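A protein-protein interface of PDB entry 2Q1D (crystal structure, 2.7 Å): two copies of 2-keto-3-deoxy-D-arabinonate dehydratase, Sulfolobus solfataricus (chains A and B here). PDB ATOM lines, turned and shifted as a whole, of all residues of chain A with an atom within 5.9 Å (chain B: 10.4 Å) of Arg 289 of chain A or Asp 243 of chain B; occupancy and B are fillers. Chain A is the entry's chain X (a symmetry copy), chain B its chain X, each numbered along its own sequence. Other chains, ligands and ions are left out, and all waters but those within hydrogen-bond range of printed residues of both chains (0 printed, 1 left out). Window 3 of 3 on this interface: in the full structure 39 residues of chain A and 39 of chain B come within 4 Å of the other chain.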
ATOM      1  N   ALA A 130      -3.494  -4.496 -11.691  1.00  0.00           N
ATOM      2  CA  ALA A 130      -2.179  -4.919 -11.232  1.00  0.00           C
ATOM      3  C   ALA A 130      -1.107  -4.804 -12.319  1.00  0.00           C
ATOM      4  O   ALA A 130      -1.325  -5.254 -13.450  1.00  0.00           O
ATOM      5  CB  ALA A 130      -2.247  -6.337 -10.679  1.00  0.00           C
ATOM      6  N   ILE A 131       0.029  -4.181 -11.969  1.00  0.00           N
ATOM      7  CA  ILE A 131       1.275  -4.296 -12.741  1.00  0.00           C
ATOM      8  C   ILE A 131       1.942  -5.615 -12.368  1.00  0.00           C
ATOM      9  O   ILE A 131       1.539  -6.225 -11.381  1.00  0.00           O
ATOM     10  CB  ILE A 131       2.241  -3.097 -12.549  1.00  0.00           C
ATOM     11  CG1 ILE A 131       2.670  -2.937 -11.085  1.00  0.00           C
ATOM     12  CG2 ILE A 131       1.607  -1.821 -13.069  1.00  0.00           C
ATOM     13  CD1 ILE A 131       3.526  -1.673 -10.800  1.00  0.00           C
ATOM     14  N   ALA A 132       2.928  -6.065 -13.151  1.00  0.00           N
ATOM     15  CA  ALA A 132       3.534  -7.383 -12.948  1.00  0.00           C
ATOM     16  C   ALA A 132       5.057  -7.338 -12.802  1.00  0.00           C
ATOM     17  O   ALA A 132       5.705  -6.421 -13.305  1.00  0.00           O
ATOM     18  CB  ALA A 132       3.148  -8.311 -14.064  1.00  0.00           C
ATOM     19  N   VAL A 133       5.621  -8.322 -12.098  1.00  0.00           N
ATOM     20  CA  VAL A 133       7.073  -8.469 -11.972  1.00  0.00           C
ATOM     21  C   VAL A 133       7.401  -9.785 -12.631  1.00  0.00           C
ATOM     22  O   VAL A 133       6.800 -10.803 -12.292  1.00  0.00           O
ATOM     23  CB  VAL A 133       7.534  -8.476 -10.478  1.00  0.00           C
ATOM     24  CG1 VAL A 133       8.995  -8.905 -10.346  1.00  0.00           C
ATOM     25  CG2 VAL A 133       7.314  -7.095  -9.833  1.00  0.00           C
ATOM     26  N   ARG A 134       8.324  -9.779 -13.584  1.00  0.00           N
ATOM     27  CA  ARG A 134       8.640 -11.000 -14.338  1.00  0.00           C
ATOM     28  C   ARG A 134       9.025 -12.125 -13.383  1.00  0.00           C
ATOM     29  O   ARG A 134       9.725 -11.908 -12.374  1.00  0.00           O
ATOM     30  CB  ARG A 134       9.791 -10.780 -15.334  1.00  0.00           C
ATOM     31  CG  ARG A 134       9.558  -9.761 -16.460  1.00  0.00           C
ATOM     32  CD  ARG A 134      10.824  -9.633 -17.335  1.00  0.00           C
ATOM     33  NE  ARG A 134      11.221 -10.945 -17.831  1.00  0.00           N
ATOM     34  CZ  ARG A 134      10.937 -11.405 -19.038  1.00  0.00           C
ATOM     35  NH1 ARG A 134      10.299 -10.635 -19.898  1.00  0.00           N
ATOM     36  NH2 ARG A 134      11.309 -12.625 -19.398  1.00  0.00           N
ATOM     37  N   SER A 135       8.578 -13.329 -13.712  1.00  0.00           N
ATOM     38  CA  SER A 135       8.860 -14.510 -12.905  1.00  0.00           C
ATOM     39  C   SER A 135      10.352 -14.625 -12.606  1.00  0.00           C
ATOM     40  O   SER A 135      10.747 -15.077 -11.529  1.00  0.00           O
ATOM     41  CB  SER A 135       8.391 -15.763 -13.645  1.00  0.00           C
ATOM     42  OG  SER A 135       9.334 -16.145 -14.634  1.00  0.00           O
ATOM     43  N   ASP A 136      11.169 -14.209 -13.573  1.00  0.00           N
ATOM     44  CA  ASP A 136      12.613 -14.357 -13.497  1.00  0.00           C
ATOM     45  C   ASP A 136      13.363 -13.046 -13.230  1.00  0.00           C
ATOM     46  O   ASP A 136      14.564 -12.956 -13.502  1.00  0.00           O
ATOM     47  CB  ASP A 136      13.137 -15.031 -14.773  1.00  0.00           C
ATOM     48  CG  ASP A 136      12.901 -14.192 -16.054  1.00  0.00           C
ATOM     49  OD1 ASP A 136      12.342 -13.057 -16.006  1.00  0.00           O
ATOM     50  OD2 ASP A 136      13.294 -14.694 -17.133  1.00  0.00           O
ATOM     51  N   TYR A 184       6.400  -6.937 -21.531  1.00  0.00           N
ATOM     52  CA  TYR A 184       5.767  -8.191 -21.049  1.00  0.00           C
ATOM     53  C   TYR A 184       4.387  -7.847 -20.449  1.00  0.00           C
ATOM     54  O   TYR A 184       4.095  -6.673 -20.177  1.00  0.00           O
ATOM     55  CB  TYR A 184       6.647  -8.923 -19.997  1.00  0.00           C
ATOM     56  CG  TYR A 184       7.010  -8.032 -18.830  1.00  0.00           C
ATOM     57  CD1 TYR A 184       6.170  -7.932 -17.726  1.00  0.00           C
ATOM     58  CD2 TYR A 184       8.163  -7.256 -18.849  1.00  0.00           C
ATOM     59  CE1 TYR A 184       6.473  -7.094 -16.652  1.00  0.00           C
ATOM     60  CE2 TYR A 184       8.482  -6.409 -17.785  1.00  0.00           C
ATOM     61  CZ  TYR A 184       7.627  -6.330 -16.683  1.00  0.00           C
ATOM     62  OH  TYR A 184       7.908  -5.487 -15.617  1.00  0.00           O
ATOM     63  N   ALA A 185       3.542  -8.851 -20.226  1.00  0.00           N
ATOM     64  CA  ALA A 185       2.199  -8.583 -19.729  1.00  0.00           C
ATOM     65  C   ALA A 185       2.271  -7.775 -18.433  1.00  0.00           C
ATOM     66  O   ALA A 185       2.939  -8.179 -17.485  1.00  0.00           O
ATOM     67  CB  ALA A 185       1.449  -9.873 -19.514  1.00  0.00           C
ATOM     68  N   GLY A 186       1.619  -6.622 -18.402  1.00  0.00           N
ATOM     69  CA  GLY A 186       1.597  -5.825 -17.197  1.00  0.00           C
ATOM     70  C   GLY A 186       2.852  -5.014 -16.952  1.00  0.00           C
ATOM     71  O   GLY A 186       3.022  -4.439 -15.875  1.00  0.00           O
ATOM     72  N   ASP A 268       5.404  -9.053  -4.540  1.00  0.00           N
ATOM     73  CA  ASP A 268       3.986  -9.355  -4.652  1.00  0.00           C
ATOM     74  C   ASP A 268       3.161  -8.574  -3.643  1.00  0.00           C
ATOM     75  O   ASP A 268       3.541  -8.481  -2.484  1.00  0.00           O
ATOM     76  CB  ASP A 268       3.757 -10.854  -4.489  1.00  0.00           C
ATOM     77  CG  ASP A 268       2.396 -11.283  -4.983  1.00  0.00           C
ATOM     78  OD1 ASP A 268       1.413 -11.127  -4.232  1.00  0.00           O
ATOM     79  OD2 ASP A 268       2.300 -11.773  -6.131  1.00  0.00           O
ATOM     80  N   LYS A 287       1.953  -7.594  -8.767  1.00  0.00           N
ATOM     81  CA  LYS A 287       1.697  -9.013  -8.762  1.00  0.00           C
ATOM     82  C   LYS A 287       2.903  -9.726  -9.388  1.00  0.00           C
ATOM     83  O   LYS A 287       3.234  -9.507 -10.557  1.00  0.00           O
ATOM     84  CB  LYS A 287       0.358  -9.286  -9.472  1.00  0.00           C
ATOM     85  CG  LYS A 287       0.158 -10.663 -10.074  1.00  0.00           C
ATOM     86  CD  LYS A 287      -0.326 -11.678  -9.043  1.00  0.00           C
ATOM     87  CE  LYS A 287      -0.134 -13.112  -9.554  1.00  0.00           C
ATOM     88  NZ  LYS A 287      -0.040 -14.064  -8.407  1.00  0.00           N
ATOM     89  N   LYS A 288       3.586 -10.536  -8.581  1.00  0.00           N
ATOM     90  CA  LYS A 288       4.725 -11.324  -9.025  1.00  0.00           C
ATOM     91  C   LYS A 288       4.241 -12.552  -9.783  1.00  0.00           C
ATOM     92  O   LYS A 288       3.396 -13.288  -9.282  1.00  0.00           O
ATOM     93  CB  LYS A 288       5.559 -11.750  -7.817  1.00  0.00           C
ATOM     94  CG  LYS A 288       6.605 -12.840  -8.098  1.00  0.00           C
ATOM     95  CD  LYS A 288       7.950 -12.256  -8.517  1.00  0.00           C
ATOM     96  CE  LYS A 288       8.951 -13.355  -8.804  1.00  0.00           C
ATOM     97  NZ  LYS A 288      10.271 -12.758  -9.136  1.00  0.00           N
ATOM     98  N   ARG A 289       4.769 -12.775 -10.984  1.00  0.00           N
ATOM     99  CA  ARG A 289       4.349 -13.921 -11.795  1.00  0.00           C
ATOM    100  C   ARG A 289       5.107 -15.178 -11.367  1.00  0.00           C
ATOM    101  O   ARG A 289       6.040 -15.100 -10.575  1.00  0.00           O
ATOM    102  CB  ARG A 289       4.552 -13.644 -13.292  1.00  0.00           C
ATOM    103  CG  ARG A 289       3.746 -12.485 -13.849  1.00  0.00           C
ATOM    104  CD  ARG A 289       2.508 -12.947 -14.600  1.00  0.00           C
ATOM    105  NE  ARG A 289       1.993 -11.875 -15.452  1.00  0.00           N
ATOM    106  CZ  ARG A 289       0.944 -11.101 -15.162  1.00  0.00           C
ATOM    107  NH1 ARG A 289       0.574 -10.145 -16.010  1.00  0.00           N
ATOM    108  NH2 ARG A 289       0.256 -11.273 -14.036  1.00  0.00           N
ATOM    109  N   ARG A 290       4.718 -16.329 -11.911  1.00  0.00           N
ATOM    110  CA  ARG A 290       5.252 -17.615 -11.457  1.00  0.00           C
ATOM    111  C   ARG A 290       5.912 -18.471 -12.568  1.00  0.00           C
ATOM    112  O   ARG A 290       5.997 -18.034 -13.719  1.00  0.00           O
ATOM    113  CB  ARG A 290       4.148 -18.374 -10.716  1.00  0.00           C
ATOM    114  CG  ARG A 290       3.892 -17.843  -9.297  1.00  0.00           C
ATOM    115  CD  ARG A 290       2.407 -17.872  -8.930  1.00  0.00           C
ATOM    116  NE  ARG A 290       1.781 -19.174  -9.202  1.00  0.00           N
ATOM    117  CZ  ARG A 290       1.506 -20.106  -8.283  1.00  0.00           C
ATOM    118  NH1 ARG A 290       1.790 -19.902  -6.999  1.00  0.00           N
ATOM    119  NH2 ARG A 290       0.935 -21.249  -8.652  1.00  0.00           N
ATOM    120  N   LYS A 291       6.375 -19.679 -12.227  1.00  0.00           N
ATOM    121  CA  LYS A 291       7.157 -20.502 -13.163  1.00  0.00           C
ATOM    122  C   LYS A 291       6.433 -21.745 -13.688  1.00  0.00           C
ATOM    123  O   LYS A 291       6.947 -22.444 -14.569  1.00  0.00           O
ATOM    124  CB  LYS A 291       8.489 -20.901 -12.523  1.00  0.00           C
ATOM    125  CG  LYS A 291       9.347 -19.717 -12.109  1.00  0.00           C
ATOM    126  CD  LYS A 291      10.807 -20.131 -11.908  1.00  0.00           C
ATOM    127  CE  LYS A 291      11.729 -18.912 -11.765  1.00  0.00           C
ATOM    128  NZ  LYS A 291      11.229 -17.904 -10.761  1.00  0.00           N
ATOM    129  N   GLU B  75       2.448  -9.244 -34.510  1.00  0.00           N
ATOM    130  CA  GLU B  75       3.727  -8.851 -33.905  1.00  0.00           C
ATOM    131  C   GLU B  75       4.886  -9.612 -34.541  1.00  0.00           C
ATOM    132  O   GLU B  75       4.791 -10.820 -34.794  1.00  0.00           O
ATOM    133  CB  GLU B  75       3.736  -9.128 -32.398  1.00  0.00           C
ATOM    134  CG  GLU B  75       2.722  -8.311 -31.612  1.00  0.00           C
ATOM    135  CD  GLU B  75       2.686  -8.621 -30.121  1.00  0.00           C
ATOM    136  OE1 GLU B  75       3.609  -9.307 -29.592  1.00  0.00           O
ATOM    137  OE2 GLU B  75       1.717  -8.153 -29.485  1.00  0.00           O
ATOM    138  N   TRP B  77       9.000 -10.362 -33.797  1.00  0.00           N
ATOM    139  CA  TRP B  77      10.058 -10.338 -32.786  1.00  0.00           C
ATOM    140  C   TRP B  77      11.311 -10.953 -33.385  1.00  0.00           C
ATOM    141  O   TRP B  77      11.231 -11.901 -34.191  1.00  0.00           O
ATOM    142  CB  TRP B  77       9.669 -11.164 -31.545  1.00  0.00           C
ATOM    143  CG  TRP B  77       8.614 -10.529 -30.687  1.00  0.00           C
ATOM    144  CD1 TRP B  77       7.267 -10.531 -30.905  1.00  0.00           C
ATOM    145  CD2 TRP B  77       8.821  -9.804 -29.472  1.00  0.00           C
ATOM    146  NE1 TRP B  77       6.622  -9.847 -29.907  1.00  0.00           N
ATOM    147  CE2 TRP B  77       7.554  -9.389 -29.013  1.00  0.00           C
ATOM    148  CE3 TRP B  77       9.953  -9.460 -28.730  1.00  0.00           C
ATOM    149  CZ2 TRP B  77       7.390  -8.646 -27.854  1.00  0.00           C
ATOM    150  CZ3 TRP B  77       9.787  -8.728 -27.576  1.00  0.00           C
ATOM    151  CH2 TRP B  77       8.516  -8.328 -27.151  1.00  0.00           C
ATOM    152  N   ARG B 112      20.567 -16.803 -20.987  1.00  0.00           N
ATOM    153  CA  ARG B 112      19.509 -15.988 -21.592  1.00  0.00           C
ATOM    154  C   ARG B 112      19.894 -15.489 -22.995  1.00  0.00           C
ATOM    155  O   ARG B 112      20.861 -14.743 -23.135  1.00  0.00           O
ATOM    156  CB  ARG B 112      19.186 -14.800 -20.671  1.00  0.00           C
ATOM    157  CG  ARG B 112      18.060 -13.914 -21.144  1.00  0.00           C
ATOM    158  CD  ARG B 112      17.817 -12.736 -20.195  1.00  0.00           C
ATOM    159  NE  ARG B 112      17.407 -13.169 -18.861  1.00  0.00           N
ATOM    160  CZ  ARG B 112      16.230 -13.716 -18.560  1.00  0.00           C
ATOM    161  NH1 ARG B 112      15.976 -14.076 -17.314  1.00  0.00           N
ATOM    162  NH2 ARG B 112      15.307 -13.913 -19.488  1.00  0.00           N
ATOM    163  N   SER B 152      -0.345 -18.670 -29.971  1.00  0.00           N
ATOM    164  CA  SER B 152      -0.196 -18.069 -28.642  1.00  0.00           C
ATOM    165  C   SER B 152       0.492 -18.971 -27.599  1.00  0.00           C
ATOM    166  O   SER B 152       0.960 -18.475 -26.574  1.00  0.00           O
ATOM    167  CB  SER B 152      -1.537 -17.533 -28.124  1.00  0.00           C
ATOM    168  OG  SER B 152      -2.497 -18.568 -28.005  1.00  0.00           O
ATOM    169  N   ILE B 237      11.920 -19.392 -28.552  1.00  0.00           N
ATOM    170  CA  ILE B 237      10.476 -19.319 -28.345  1.00  0.00           C
ATOM    171  C   ILE B 237      10.119 -19.250 -26.863  1.00  0.00           C
ATOM    172  O   ILE B 237       9.266 -18.447 -26.466  1.00  0.00           O
ATOM    173  CB  ILE B 237       9.739 -20.507 -29.002  1.00  0.00           C
ATOM    174  CG1 ILE B 237       9.935 -20.474 -30.520  1.00  0.00           C
ATOM    175  CG2 ILE B 237       8.254 -20.480 -28.638  1.00  0.00           C
ATOM    176  CD1 ILE B 237       9.196 -21.542 -31.273  1.00  0.00           C
ATOM    177  N   GLN B 238      10.781 -20.084 -26.057  1.00  0.00           N
ATOM    178  CA  GLN B 238      10.567 -20.149 -24.601  1.00  0.00           C
ATOM    179  C   GLN B 238      10.808 -18.805 -23.897  1.00  0.00           C
ATOM    180  O   GLN B 238       9.995 -18.371 -23.082  1.00  0.00           O
ATOM    181  CB  GLN B 238      11.463 -21.240 -24.011  1.00  0.00           C
ATOM    182  CG  GLN B 238      11.217 -21.626 -22.541  1.00  0.00           C
ATOM    183  CD  GLN B 238      12.500 -22.118 -21.848  1.00  0.00           C
ATOM    184  OE1 GLN B 238      12.979 -21.491 -20.903  1.00  0.00           O
ATOM    185  NE2 GLN B 238      13.073 -23.215 -22.344  1.00  0.00           N
ATOM    186  N   TYR B 239      11.914 -18.146 -24.225  1.00  0.00           N
ATOM    187  CA  TYR B 239      12.213 -16.816 -23.677  1.00  0.00           C
ATOM    188  C   TYR B 239      11.330 -15.707 -24.245  1.00  0.00           C
ATOM    189  O   TYR B 239      11.049 -14.713 -23.558  1.00  0.00           O
ATOM    190  CB  TYR B 239      13.695 -16.479 -23.844  1.00  0.00           C
ATOM    191  CG  TYR B 239      14.551 -17.131 -22.785  1.00  0.00           C
ATOM    192  CD1 TYR B 239      15.125 -18.397 -22.996  1.00  0.00           C
ATOM    193  CD2 TYR B 239      14.758 -16.501 -21.547  1.00  0.00           C
ATOM    194  CE1 TYR B 239      15.904 -19.005 -22.015  1.00  0.00           C
ATOM    195  CE2 TYR B 239      15.526 -17.101 -20.552  1.00  0.00           C
ATOM    196  CZ  TYR B 239      16.096 -18.352 -20.793  1.00  0.00           C
ATOM    197  OH  TYR B 239      16.860 -18.938 -19.807  1.00  0.00           O
ATOM    198  N   LEU B 240      10.894 -15.878 -25.493  1.00  0.00           N
ATOM    199  CA  LEU B 240       9.967 -14.934 -26.097  1.00  0.00           C
ATOM    200  C   LEU B 240       8.662 -14.900 -25.316  1.00  0.00           C
ATOM    201  O   LEU B 240       8.213 -13.819 -24.918  1.00  0.00           O
ATOM    202  CB  LEU B 240       9.686 -15.265 -27.564  1.00  0.00           C
ATOM    203  CG  LEU B 240       8.521 -14.498 -28.205  1.00  0.00           C
ATOM    204  CD1 LEU B 240       8.822 -13.006 -28.353  1.00  0.00           C
ATOM    205  CD2 LEU B 240       8.128 -15.115 -29.524  1.00  0.00           C
ATOM    206  N   ILE B 241       8.076 -16.080 -25.088  1.00  0.00           N
ATOM    207  CA  ILE B 241       6.728 -16.165 -24.510  1.00  0.00           C
ATOM    208  C   ILE B 241       6.669 -16.085 -22.991  1.00  0.00           C
ATOM    209  O   ILE B 241       5.590 -15.925 -22.436  1.00  0.00           O
ATOM    210  CB  ILE B 241       5.929 -17.395 -25.010  1.00  0.00           C
ATOM    211  CG1 ILE B 241       6.381 -18.684 -24.308  1.00  0.00           C
ATOM    212  CG2 ILE B 241       6.020 -17.494 -26.536  1.00  0.00           C
ATOM    213  CD1 ILE B 241       5.600 -19.947 -24.725  1.00  0.00           C
ATOM    214  N   ARG B 242       7.823 -16.171 -22.327  1.00  0.00           N
ATOM    215  CA  ARG B 242       7.873 -16.137 -20.862  1.00  0.00           C
ATOM    216  C   ARG B 242       7.280 -14.844 -20.301  1.00  0.00           C
ATOM    217  O   ARG B 242       7.826 -13.759 -20.540  1.00  0.00           O
ATOM    218  CB  ARG B 242       9.302 -16.316 -20.359  1.00  0.00           C
ATOM    219  CG  ARG B 242       9.446 -16.047 -18.873  1.00  0.00           C
ATOM    220  CD  ARG B 242      10.866 -16.188 -18.429  1.00  0.00           C
ATOM    221  NE  ARG B 242      11.339 -17.563 -18.611  1.00  0.00           N
ATOM    222  CZ  ARG B 242      12.479 -18.044 -18.113  1.00  0.00           C
ATOM    223  NH1 ARG B 242      13.273 -17.262 -17.380  1.00  0.00           N
ATOM    224  NH2 ARG B 242      12.823 -19.307 -18.354  1.00  0.00           N
ATOM    225  N   ASP B 243       6.175 -14.978 -19.557  1.00  0.00           N
ATOM    226  CA  ASP B 243       5.409 -13.846 -19.013  1.00  0.00           C
ATOM    227  C   ASP B 243       4.954 -12.858 -20.085  1.00  0.00           C
ATOM    228  O   ASP B 243       4.506 -11.751 -19.774  1.00  0.00           O
ATOM    229  CB  ASP B 243       6.222 -13.081 -17.956  1.00  0.00           C
ATOM    230  CG  ASP B 243       6.620 -13.941 -16.783  1.00  0.00           C
ATOM    231  OD1 ASP B 243       5.782 -14.744 -16.309  1.00  0.00           O
ATOM    232  OD2 ASP B 243       7.776 -13.796 -16.328  1.00  0.00           O
ATOM    233  N   ASN B 244       5.094 -13.250 -21.344  1.00  0.00           N
ATOM    234  CA  ASN B 244       4.879 -12.348 -22.459  1.00  0.00           C
ATOM    235  C   ASN B 244       3.911 -12.993 -23.423  1.00  0.00           C
ATOM    236  O   ASN B 244       4.293 -13.809 -24.251  1.00  0.00           O
ATOM    237  CB  ASN B 244       6.208 -12.052 -23.141  1.00  0.00           C
ATOM    238  CG  ASN B 244       6.122 -10.916 -24.132  1.00  0.00           C
ATOM    239  OD1 ASN B 244       5.426  -9.922 -23.905  1.00  0.00           O
ATOM    240  ND2 ASN B 244       6.850 -11.048 -25.239  1.00  0.00           N
ATOM    241  N   PRO B 245       2.636 -12.624 -23.319  1.00  0.00           N
ATOM    242  CA  PRO B 245       1.629 -13.301 -24.142  1.00  0.00           C
ATOM    243  C   PRO B 245       1.728 -12.797 -25.587  1.00  0.00           C
ATOM    244  O   PRO B 245       1.732 -11.580 -25.815  1.00  0.00           O
ATOM    245  CB  PRO B 245       0.306 -12.860 -23.506  1.00  0.00           C
ATOM    246  CG  PRO B 245       0.617 -11.437 -22.957  1.00  0.00           C
ATOM    247  CD  PRO B 245       2.076 -11.531 -22.491  1.00  0.00           C
ATOM    248  N   ILE B 246       1.840 -13.724 -26.536  1.00  0.00           N
ATOM    249  CA  ILE B 246       1.856 -13.373 -27.941  1.00  0.00           C
ATOM    250  C   ILE B 246       0.540 -13.751 -28.622  1.00  0.00           C
ATOM    251  O   ILE B 246      -0.085 -14.745 -28.250  1.00  0.00           O
ATOM    252  CB  ILE B 246       3.064 -14.003 -28.688  1.00  0.00           C
ATOM    253  CG1 ILE B 246       3.046 -15.535 -28.602  1.00  0.00           C
ATOM    254  CG2 ILE B 246       4.396 -13.376 -28.201  1.00  0.00           C
ATOM    255  CD1 ILE B 246       4.006 -16.226 -29.561  1.00  0.00           C
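The side-chain carboxylate (OD2) of Asp 136 of chain A is in salt-bridge range of the guanidinium group (NH1) of Arg 112 of chain B, at 2.8 Å. NH1 of Arg 242 of chain B is in salt-bridge range of OD2 of Asp 136 of chain A, 2.6 Å away. The backbone NH (N) of Ser 135 of chain A is in hydrogen-bond range of the side-chain carboxylate (OD2) of Asp 243 of chain B (2.8 Å). O of Asp 243 of chain B sits at hydrogen-bond distance from N of Ala 185 of chain A (3.1 Å).
The side-chain amide nitrogen (ND2) of Asn 244 of chain B is in hydrogen-bond range of the backbone carbonyl oxygen (O) of Leu 240 of chain B (3.1 Å). The backbone carbonyl oxygen (O) of Ala 132 of chain A sits at hydrogen-bond distance from the side-chain hydroxyl (OH) of Tyr 184 of chain A, 3.3 Å away. The side-chain carboxylate (OD1) of Asp 136 of chain A is in salt-bridge range of the guanidinium group (NE) of Arg 134 of chain A (3.0 Å). O of Arg 134 of chain A lies within hydrogen-bond range of NZ of Lys 288 of chain A, 3.4 Å away. The side-chain amino group (NZ) of Lys 288 of chain A sits at hydrogen-bond distance from the backbone carbonyl oxygen (O) of Ser 135 of chain A (3.4 Å). O of Ala 185 of chain A lies within hydrogen-bond range of NH1 of Arg 289 of chain A, at 3.4 Å.
Among the printed residues, merely in contact across the chains: Arg 134 of chain A with Arg 242 of chain B, Arg 134 of chain A with Asp 243 of chain B, Tyr 184 of chain A with Asp 243 of chain B, Tyr 184 of chain A with Asn 244 of chain B, Ala 185 of chain A with Pro 245 of chain B and Arg 289 of chain A with Asp 243 of chain B.
Arg 289 of chain A touches just one residue of chain B: Asp 243 (3.4 Å). Asp 243 of chain B touches five residues of chain A. Ser 135 of chain A touches just one residue of chain B: Asp 243 (2.8 Å). Ala 185 of chain A touches just these residues of chain B: Asp 243 and Pro 245. No residue of chain B comes within 4 Å of Gly 186 of chain A. No residue of chain B comes within 4 Å of Lys 288 of chain A. Printed residues of chain A within 4 Å of Asn 244 of chain B: Tyr 184. Of the printed residues of chain A, Arg 242 of chain B touches Arg 134 (3.7 Å) and Asp 136 (2.6 Å). Of the printed residues of chain A, Pro 245 of chain B touches Ala 185. Ser 152 of chain B touches none of the printed residues of chain A. The nearest printed residue of chain B that does not touch Tyr 184 of chain A is Pro 245 of chain B (4.8 Å).
Of the 14 printed residues of chain B, 5 touch a printed residue of chain A. Hydrophobic or aromatic side chains of chain B within 4 Å of the printed part of chain A: Pro 245. Of the 16 printed residues of chain A, 6 touch a printed residue of chain B. Among the printed residues, 10 pairs touch across the chains.
No position is printed for both chains.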
